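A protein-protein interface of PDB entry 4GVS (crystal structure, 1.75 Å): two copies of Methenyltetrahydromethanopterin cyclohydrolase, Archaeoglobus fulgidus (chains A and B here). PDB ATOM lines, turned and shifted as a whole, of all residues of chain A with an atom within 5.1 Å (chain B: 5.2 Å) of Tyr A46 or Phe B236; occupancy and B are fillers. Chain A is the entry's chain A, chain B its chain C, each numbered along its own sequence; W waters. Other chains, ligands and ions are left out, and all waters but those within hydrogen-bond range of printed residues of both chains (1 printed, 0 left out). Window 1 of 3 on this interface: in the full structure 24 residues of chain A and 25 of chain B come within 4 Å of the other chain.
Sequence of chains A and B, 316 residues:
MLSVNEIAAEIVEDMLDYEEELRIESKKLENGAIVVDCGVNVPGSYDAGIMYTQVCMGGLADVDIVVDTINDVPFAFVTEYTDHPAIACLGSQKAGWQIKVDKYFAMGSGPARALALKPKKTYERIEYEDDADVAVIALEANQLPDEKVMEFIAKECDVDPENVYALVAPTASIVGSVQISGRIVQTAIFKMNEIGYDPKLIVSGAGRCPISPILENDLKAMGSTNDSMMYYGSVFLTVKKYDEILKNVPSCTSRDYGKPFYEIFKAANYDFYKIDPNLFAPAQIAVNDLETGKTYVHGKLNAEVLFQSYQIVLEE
Water W1 lies within hydrogen-bond range of OG of Ser B204 (2.6 Å), OH of Tyr A46 (2.8 Å) and OG1 of Thr B238 (2.9 Å).
OD1 of Asp A47 sits at hydrogen-bond distance from OH of Tyr B81 (2.7 Å).
The side-chain carboxylate of Asp B83 sits at hydrogen-bond distance from the backbone NH of Tyr A46 (2.9 Å).
Of the printed residues of chain B, Tyr A46 touches Tyr B81, Asp B83, Ala B206 and Phe B236.
Of chain A, only Tyr A46, Pro A74 and Phe A75 come within 4 Å of Phe B236.
Printed residues of chain A within 4 Å of Ala B206: Tyr A46.
Of the printed residues of chain B, Ile A65 touches Tyr B81 (3.9 Å).
Gly B205 touches none of the printed residues of chain A.
The nearest printed residue of chain B that does not touch Tyr A46 is Ser B204 (4.01 Å).
No position is printed for both chains.
Of the 15 pairs that touch across the chains among the printed residues, none has its exchanged pair printed and touching as well.
Ser A45 touches Asp B83.
Tyr A46 touches Tyr B81 (CB to CE2, 3.6 Å).
Tyr A46 touches Ala B206 (OH to CB, 3.99 Å).
Phe B236 touches Tyr A46 (CD2 to OH, 3.7 Å).
CD1 of Ile A50 touches OH of Tyr B81, at 3.3 Å.
Pro A74 touches Ser B234 (CB to CB, 3.7 Å).
Phe B236 touches Pro A74.
O of Pro A74 touches CB of Ala B286 (3.7 Å).
Phe B236 touches Phe A75 (CE1 to CD2, 3.8 Å).
Thr B295 touches Pro A213.
Of the 15 printed residues of chain A, 8 touch a printed residue of chain B.
Among the printed residues, 15 pairs touch across the chains.
Among the printed residues, no Asp or Glu carboxylate lies within 4 Å of a Lys or Arg side-chain nitrogen of the other chain.
The backbone carbonyl oxygen of Leu B237 sits at hydrogen-bond distance from the backbone NH of Asn B288.
The side-chain hydroxyl (OG) of Ser A45 is in hydrogen-bond range of the backbone NH (N) of Ala A48, 3.0 Å away.
The backbone carbonyl oxygen of Ala B206 lies within hydrogen-bond range of the backbone NH of Phe B236, 2.8 Å away.
The backbone carbonyl oxygen of Val B235 is in hydrogen-bond range of the backbone NH of Ala B286, at 2.9 Å.
The backbone carbonyl oxygen (O) of Ala B286 lies within hydrogen-bond range of the backbone NH (N) of Leu B237, at 2.8 Å.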
ATOM      1  N   GLY A  44      30.946 -10.992  10.099  1.00  0.00           N
ATOM      2  CA  GLY A  44      32.197 -11.318  10.851  1.00  0.00           C
ATOM      3  C   GLY A  44      31.920 -12.476  11.830  1.00  0.00           C
ATOM      4  O   GLY A  44      30.933 -13.230  11.664  1.00  0.00           O
ATOM      5  N   SER A  45      32.756 -12.597  12.852  1.00  0.00           N
ATOM      6  CA  SER A  45      32.755 -13.837  13.684  1.00  0.00           C
ATOM      7  C   SER A  45      33.603 -13.593  14.875  1.00  0.00           C
ATOM      8  O   SER A  45      34.403 -12.647  14.892  1.00  0.00           O
ATOM      9  CB  SER A  45      33.315 -15.033  12.900  1.00  0.00           C
ATOM     10  OG  SER A  45      34.615 -14.801  12.348  1.00  0.00           O
ATOM     11  N   TYR A  46      33.462 -14.458  15.871  1.00  0.00           N
ATOM     12  CA  TYR A  46      34.374 -14.363  17.008  1.00  0.00           C
ATOM     13  C   TYR A  46      35.837 -14.507  16.575  1.00  0.00           C
ATOM     14  O   TYR A  46      36.675 -13.742  17.060  1.00  0.00           O
ATOM     15  CB  TYR A  46      34.036 -15.489  17.986  1.00  0.00           C
ATOM     16  CG  TYR A  46      32.851 -15.246  18.849  1.00  0.00           C
ATOM     17  CD1 TYR A  46      31.743 -16.163  18.831  1.00  0.00           C
ATOM     18  CD2 TYR A  46      32.817 -14.176  19.774  1.00  0.00           C
ATOM     19  CE1 TYR A  46      30.650 -15.975  19.650  1.00  0.00           C
ATOM     20  CE2 TYR A  46      31.760 -14.034  20.648  1.00  0.00           C
ATOM     21  CZ  TYR A  46      30.650 -14.927  20.563  1.00  0.00           C
ATOM     22  OH  TYR A  46      29.573 -14.700  21.401  1.00  0.00           O
ATOM     23  N   ASP A  47      36.130 -15.469  15.701  1.00  0.00           N
ATOM     24  CA  ASP A  47      37.504 -15.654  15.268  1.00  0.00           C
ATOM     25  C   ASP A  47      38.012 -14.474  14.444  1.00  0.00           C
ATOM     26  O   ASP A  47      39.188 -14.061  14.587  1.00  0.00           O
ATOM     27  CB  ASP A  47      37.655 -16.936  14.489  1.00  0.00           C
ATOM     28  CG  ASP A  47      37.860 -18.138  15.420  1.00  0.00           C
ATOM     29  OD1 ASP A  47      38.218 -17.911  16.580  1.00  0.00           O
ATOM     30  OD2 ASP A  47      37.805 -19.242  14.896  1.00  0.00           O
ATOM     31  N   ALA A  48      37.115 -13.877  13.667  1.00  0.00           N
ATOM     32  CA  ALA A  48      37.528 -12.647  12.931  1.00  0.00           C
ATOM     33  C   ALA A  48      37.844 -11.557  13.921  1.00  0.00           C
ATOM     34  O   ALA A  48      38.825 -10.778  13.730  1.00  0.00           O
ATOM     35  CB  ALA A  48      36.421 -12.166  11.964  1.00  0.00           C
ATOM     36  N   GLY A  49      37.077 -11.501  15.010  1.00  0.00           N
ATOM     37  CA  GLY A  49      37.268 -10.493  16.083  1.00  0.00           C
ATOM     38  C   GLY A  49      38.633 -10.730  16.759  1.00  0.00           C
ATOM     39  O   GLY A  49      39.364  -9.763  17.084  1.00  0.00           O
ATOM     40  N   ILE A  50      38.957 -11.985  17.073  1.00  0.00           N
ATOM     41  CA  ILE A  50      40.280 -12.258  17.697  1.00  0.00           C
ATOM     42  C   ILE A  50      41.424 -11.827  16.743  1.00  0.00           C
ATOM     43  O   ILE A  50      42.403 -11.147  17.194  1.00  0.00           O
ATOM     44  CB  ILE A  50      40.411 -13.784  18.002  1.00  0.00           C
ATOM     45  CG1 ILE A  50      39.399 -14.117  19.134  1.00  0.00           C
ATOM     46  CG2 ILE A  50      41.874 -14.101  18.346  1.00  0.00           C
ATOM     47  CD1 ILE A  50      39.340 -15.673  19.393  1.00  0.00           C
ATOM     48  N   ILE A  65      39.413 -16.317  23.393  1.00  0.00           N
ATOM     49  CA  ILE A  65      38.071 -16.165  23.983  1.00  0.00           C
ATOM     50  C   ILE A  65      37.760 -17.394  24.863  1.00  0.00           C
ATOM     51  O   ILE A  65      38.068 -18.550  24.457  1.00  0.00           O
ATOM     52  CB  ILE A  65      36.967 -15.961  22.907  1.00  0.00           C
ATOM     53  CG1 ILE A  65      37.170 -14.557  22.275  1.00  0.00           C
ATOM     54  CG2 ILE A  65      35.568 -16.074  23.478  1.00  0.00           C
ATOM     55  CD1 ILE A  65      36.325 -14.386  21.004  1.00  0.00           C
ATOM     56  N   PRO A  74      26.042 -16.204  31.559  1.00  0.00           N
ATOM     57  CA  PRO A  74      27.130 -16.557  30.672  1.00  0.00           C
ATOM     58  C   PRO A  74      27.505 -15.421  29.710  1.00  0.00           C
ATOM     59  O   PRO A  74      26.628 -14.789  29.147  1.00  0.00           O
ATOM     60  CB  PRO A  74      26.553 -17.719  29.839  1.00  0.00           C
ATOM     61  CG  PRO A  74      25.092 -17.788  30.157  1.00  0.00           C
ATOM     62  CD  PRO A  74      24.742 -16.811  31.209  1.00  0.00           C
ATOM     63  N   PHE A  75      28.817 -15.160  29.540  1.00  0.00           N
ATOM     64  CA  PHE A  75      29.316 -14.237  28.553  1.00  0.00           C
ATOM     65  C   PHE A  75      30.588 -14.867  27.945  1.00  0.00           C
ATOM     66  O   PHE A  75      31.282 -15.653  28.603  1.00  0.00           O
ATOM     67  CB  PHE A  75      29.754 -12.867  29.161  1.00  0.00           C
ATOM     68  CG  PHE A  75      28.603 -12.068  29.727  1.00  0.00           C
ATOM     69  CD1 PHE A  75      28.256 -12.207  31.087  1.00  0.00           C
ATOM     70  CD2 PHE A  75      27.797 -11.281  28.863  1.00  0.00           C
ATOM     71  CE1 PHE A  75      27.211 -11.495  31.592  1.00  0.00           C
ATOM     72  CE2 PHE A  75      26.700 -10.575  29.369  1.00  0.00           C
ATOM     73  CZ  PHE A  75      26.422 -10.688  30.744  1.00  0.00           C
ATOM     74  N   ALA A  76      30.912 -14.406  26.737  1.00  0.00           N
ATOM     75  CA  ALA A  76      32.194 -14.696  26.135  1.00  0.00           C
ATOM     76  C   ALA A  76      33.146 -13.603  26.693  1.00  0.00           C
ATOM     77  O   ALA A  76      32.735 -12.457  26.842  1.00  0.00           O
ATOM     78  CB  ALA A  76      32.049 -14.583  24.598  1.00  0.00           C
ATOM     79  N   ILE A 174      30.005  -7.989  15.933  1.00  0.00           N
ATOM     80  CA  ILE A 174      30.805  -8.911  16.789  1.00  0.00           C
ATOM     81  C   ILE A 174      32.253  -8.562  16.739  1.00  0.00           C
ATOM     82  O   ILE A 174      32.889  -8.546  17.781  1.00  0.00           O
ATOM     83  CB  ILE A 174      30.542 -10.418  16.538  1.00  0.00           C
ATOM     84  CG1 ILE A 174      31.153 -11.275  17.686  1.00  0.00           C
ATOM     85  CG2 ILE A 174      31.115 -10.908  15.227  1.00  0.00           C
ATOM     86  CD1 ILE A 174      30.636 -10.904  19.094  1.00  0.00           C
ATOM     87  N   VAL A 178      34.389  -7.685  20.167  1.00  0.00           N
ATOM     88  CA  VAL A 178      35.619  -8.434  20.516  1.00  0.00           C
ATOM     89  C   VAL A 178      36.828  -7.471  20.575  1.00  0.00           C
ATOM     90  O   VAL A 178      37.561  -7.405  21.559  1.00  0.00           O
ATOM     91  CB  VAL A 178      35.903  -9.543  19.554  1.00  0.00           C
ATOM     92  CG1 VAL A 178      37.254 -10.204  19.956  1.00  0.00           C
ATOM     93  CG2 VAL A 178      34.748 -10.581  19.609  1.00  0.00           C
ATOM     94  N   ILE A 211      33.041  -9.703  26.681  1.00  0.00           N
ATOM     95  CA  ILE A 211      32.668  -9.193  25.368  1.00  0.00           C
ATOM     96  C   ILE A 211      31.208  -8.706  25.370  1.00  0.00           C
ATOM     97  O   ILE A 211      30.278  -9.440  25.705  1.00  0.00           O
ATOM     98  CB  ILE A 211      32.875 -10.308  24.329  1.00  0.00           C
ATOM     99  CG1 ILE A 211      34.379 -10.606  24.247  1.00  0.00           C
ATOM    100  CG2 ILE A 211      32.439  -9.853  22.936  1.00  0.00           C
ATOM    101  CD1 ILE A 211      34.650 -11.976  23.517  1.00  0.00           C
ATOM    102  N   PRO A 213      27.504  -7.680  24.463  1.00  0.00           N
ATOM    103  CA  PRO A 213      26.476  -8.007  23.477  1.00  0.00           C
ATOM    104  C   PRO A 213      26.387  -6.848  22.529  1.00  0.00           C
ATOM    105  O   PRO A 213      26.841  -5.711  22.873  1.00  0.00           O
ATOM    106  CB  PRO A 213      25.176  -8.036  24.279  1.00  0.00           C
ATOM    107  CG  PRO A 213      25.569  -8.172  25.718  1.00  0.00           C
ATOM    108  CD  PRO A 213      26.970  -7.661  25.846  1.00  0.00           C
ATOM    109  N   TYR B  81      32.845 -22.094  20.791  1.00  0.00           N
ATOM    110  CA  TYR B  81      31.953 -21.114  20.109  1.00  0.00           C
ATOM    111  C   TYR B  81      31.957 -21.360  18.630  1.00  0.00           C
ATOM    112  O   TYR B  81      32.892 -21.967  18.071  1.00  0.00           O
ATOM    113  CB  TYR B  81      32.349 -19.602  20.445  1.00  0.00           C
ATOM    114  CG  TYR B  81      33.775 -19.311  20.146  1.00  0.00           C
ATOM    115  CD1 TYR B  81      34.801 -19.425  21.166  1.00  0.00           C
ATOM    116  CD2 TYR B  81      34.185 -18.958  18.867  1.00  0.00           C
ATOM    117  CE1 TYR B  81      36.125 -19.169  20.843  1.00  0.00           C
ATOM    118  CE2 TYR B  81      35.506 -18.672  18.587  1.00  0.00           C
ATOM    119  CZ  TYR B  81      36.490 -18.869  19.545  1.00  0.00           C
ATOM    120  OH  TYR B  81      37.808 -18.597  19.205  1.00  0.00           O
ATOM    121  N   THR B  82      30.867 -20.896  18.000  1.00  0.00           N
ATOM    122  CA  THR B  82      30.744 -21.031  16.567  1.00  0.00           C
ATOM    123  C   THR B  82      29.962 -19.885  15.969  1.00  0.00           C
ATOM    124  O   THR B  82      29.028 -19.409  16.574  1.00  0.00           O
ATOM    125  CB  THR B  82      30.082 -22.389  16.188  1.00  0.00           C
ATOM    126  OG1 THR B  82      29.960 -22.506  14.746  1.00  0.00           O
ATOM    127  CG2 THR B  82      28.660 -22.554  16.828  1.00  0.00           C
ATOM    128  N   ASP B  83      30.308 -19.497  14.741  1.00  0.00           N
ATOM    129  CA  ASP B  83      29.502 -18.520  14.009  1.00  0.00           C
ATOM    130  C   ASP B  83      28.750 -19.181  12.837  1.00  0.00           C
ATOM    131  O   ASP B  83      28.289 -18.490  11.927  1.00  0.00           O
ATOM    132  CB  ASP B  83      30.406 -17.409  13.501  1.00  0.00           C
ATOM    133  CG  ASP B  83      30.737 -16.426  14.624  1.00  0.00           C
ATOM    134  OD1 ASP B  83      31.746 -16.668  15.321  1.00  0.00           O
ATOM    135  OD2 ASP B  83      29.954 -15.512  14.851  1.00  0.00           O
ATOM    136  N   SER B 204      25.080 -16.751  16.264  1.00  0.00           N
ATOM    137  CA  SER B 204      26.329 -17.387  16.804  1.00  0.00           C
ATOM    138  C   SER B 204      26.001 -17.916  18.196  1.00  0.00           C
ATOM    139  O   SER B 204      24.951 -17.592  18.768  1.00  0.00           O
ATOM    140  CB  SER B 204      27.475 -16.333  16.836  1.00  0.00           C
ATOM    141  OG  SER B 204      27.193 -15.284  17.743  1.00  0.00           O
ATOM    142  N   GLY B 205      26.859 -18.756  18.759  1.00  0.00           N
ATOM    143  CA  GLY B 205      26.649 -19.075  20.175  1.00  0.00           C
ATOM    144  C   GLY B 205      28.009 -19.494  20.739  1.00  0.00           C
ATOM    145  O   GLY B 205      28.893 -19.950  20.013  1.00  0.00           O
ATOM    146  N   ALA B 206      28.108 -19.425  22.056  1.00  0.00           N
ATOM    147  CA  ALA B 206      29.365 -19.662  22.749  1.00  0.00           C
ATOM    148  C   ALA B 206      28.957 -20.321  24.063  1.00  0.00           C
ATOM    149  O   ALA B 206      28.007 -19.860  24.730  1.00  0.00           O
ATOM    150  CB  ALA B 206      30.066 -18.314  23.007  1.00  0.00           C
ATOM    151  N   GLY B 207      29.632 -21.394  24.426  1.00  0.00           N
ATOM    152  CA  GLY B 207      29.137 -22.191  25.566  1.00  0.00           C
ATOM    153  C   GLY B 207      30.257 -22.714  26.423  1.00  0.00           C
ATOM    154  O   GLY B 207      31.435 -22.798  25.965  1.00  0.00           O
ATOM    155  N   SER B 234      26.217 -23.619  30.141  1.00  0.00           N
ATOM    156  CA  SER B 234      25.795 -22.218  29.975  1.00  0.00           C
ATOM    157  C   SER B 234      26.087 -21.825  28.547  1.00  0.00           C
ATOM    158  O   SER B 234      27.175 -22.132  28.043  1.00  0.00           O
ATOM    159  CB  SER B 234      26.546 -21.232  30.897  1.00  0.00           C
ATOM    160  OG  SER B 234      26.572 -21.657  32.247  1.00  0.00           O
ATOM    161  N   VAL B 235      25.159 -21.078  27.930  1.00  0.00           N
ATOM    162  CA  VAL B 235      25.346 -20.639  26.547  1.00  0.00           C
ATOM    163  C   VAL B 235      24.999 -19.155  26.395  1.00  0.00           C
ATOM    164  O   VAL B 235      23.934 -18.726  26.843  1.00  0.00           O
ATOM    165  CB  VAL B 235      24.477 -21.479  25.604  1.00  0.00           C
ATOM    166  CG1 VAL B 235      24.812 -21.235  24.123  1.00  0.00           C
ATOM    167  CG2 VAL B 235      24.628 -22.974  25.900  1.00  0.00           C
ATOM    168  N   PHE B 236      25.899 -18.388  25.766  1.00  0.00           N
ATOM    169  CA  PHE B 236      25.595 -17.084  25.310  1.00  0.00           C
ATOM    170  C   PHE B 236      25.300 -17.160  23.782  1.00  0.00           C
ATOM    171  O   PHE B 236      26.148 -17.714  23.018  1.00  0.00           O
ATOM    172  CB  PHE B 236      26.800 -16.186  25.557  1.00  0.00           C
ATOM    173  CG  PHE B 236      26.557 -14.741  25.122  1.00  0.00           C
ATOM    174  CD1 PHE B 236      26.187 -13.763  26.052  1.00  0.00           C
ATOM    175  CD2 PHE B 236      26.756 -14.356  23.785  1.00  0.00           C
ATOM    176  CE1 PHE B 236      25.996 -12.416  25.668  1.00  0.00           C
ATOM    177  CE2 PHE B 236      26.544 -13.009  23.366  1.00  0.00           C
ATOM    178  CZ  PHE B 236      26.190 -12.030  24.333  1.00  0.00           C
ATOM    179  N   LEU B 237      24.128 -16.657  23.359  1.00  0.00           N
ATOM    180  CA  LEU B 237      23.632 -16.832  21.964  1.00  0.00           C
ATOM    181  C   LEU B 237      23.321 -15.483  21.406  1.00  0.00           C
ATOM    182  O   LEU B 237      22.880 -14.615  22.156  1.00  0.00           O
ATOM    183  CB  LEU B 237      22.310 -17.622  22.006  1.00  0.00           C
ATOM    184  CG  LEU B 237      22.453 -19.070  22.422  1.00  0.00           C
ATOM    185  CD1 LEU B 237      21.207 -19.545  23.151  1.00  0.00           C
ATOM    186  CD2 LEU B 237      22.677 -19.994  21.210  1.00  0.00           C
ATOM    187  N   THR B 238      23.547 -15.284  20.105  1.00  0.00           N
ATOM    188  CA  THR B 238      23.154 -14.038  19.481  1.00  0.00           C
ATOM    189  C   THR B 238      22.099 -14.395  18.421  1.00  0.00           C
ATOM    190  O   THR B 238      22.286 -15.335  17.669  1.00  0.00           O
ATOM    191  CB  THR B 238      24.377 -13.374  18.843  1.00  0.00           C
ATOM    192  OG1 THR B 238      25.310 -13.074  19.897  1.00  0.00           O
ATOM    193  CG2 THR B 238      24.012 -12.014  18.159  1.00  0.00           C
ATOM    194  N   ALA B 286      21.989 -16.817  27.836  1.00  0.00           N
ATOM    195  CA  ALA B 286      21.810 -15.389  27.686  1.00  0.00           C
ATOM    196  C   ALA B 286      21.645 -15.199  26.199  1.00  0.00           C
ATOM    197  O   ALA B 286      22.502 -15.720  25.393  1.00  0.00           O
ATOM    198  CB  ALA B 286      23.031 -14.612  28.189  1.00  0.00           C
ATOM    199  N   ASN B 288      21.331 -12.462  23.219  1.00  0.00           N
ATOM    200  CA  ASN B 288      21.550 -11.104  22.741  1.00  0.00           C
ATOM    201  C   ASN B 288      20.661 -10.988  21.512  1.00  0.00           C
ATOM    202  O   ASN B 288      20.931 -11.604  20.469  1.00  0.00           O
ATOM    203  CB  ASN B 288      23.035 -10.890  22.375  1.00  0.00           C
ATOM    204  CG  ASN B 288      23.305  -9.552  21.720  1.00  0.00           C
ATOM    205  OD1 ASN B 288      22.525  -8.576  21.880  1.00  0.00           O
ATOM    206  ND2 ASN B 288      24.393  -9.477  20.992  1.00  0.00           N
ATOM    207  N   THR B 295      19.545  -8.198  26.045  1.00  0.00           N
ATOM    208  CA  THR B 295      20.062  -9.566  26.189  1.00  0.00           C
ATOM    209  C   THR B 295      19.289 -10.228  27.288  1.00  0.00           C
ATOM    210  O   THR B 295      19.328  -9.801  28.456  1.00  0.00           O
ATOM    211  CB  THR B 295      21.587  -9.641  26.517  1.00  0.00           C
ATOM    212  OG1 THR B 295      22.323  -9.269  25.350  1.00  0.00           O
ATOM    213  CG2 THR B 295      21.989 -11.092  26.839  1.00  0.00           C
HETATM  214  O   HOH W   1      27.057 -15.370  20.364  1.00  0.00           O
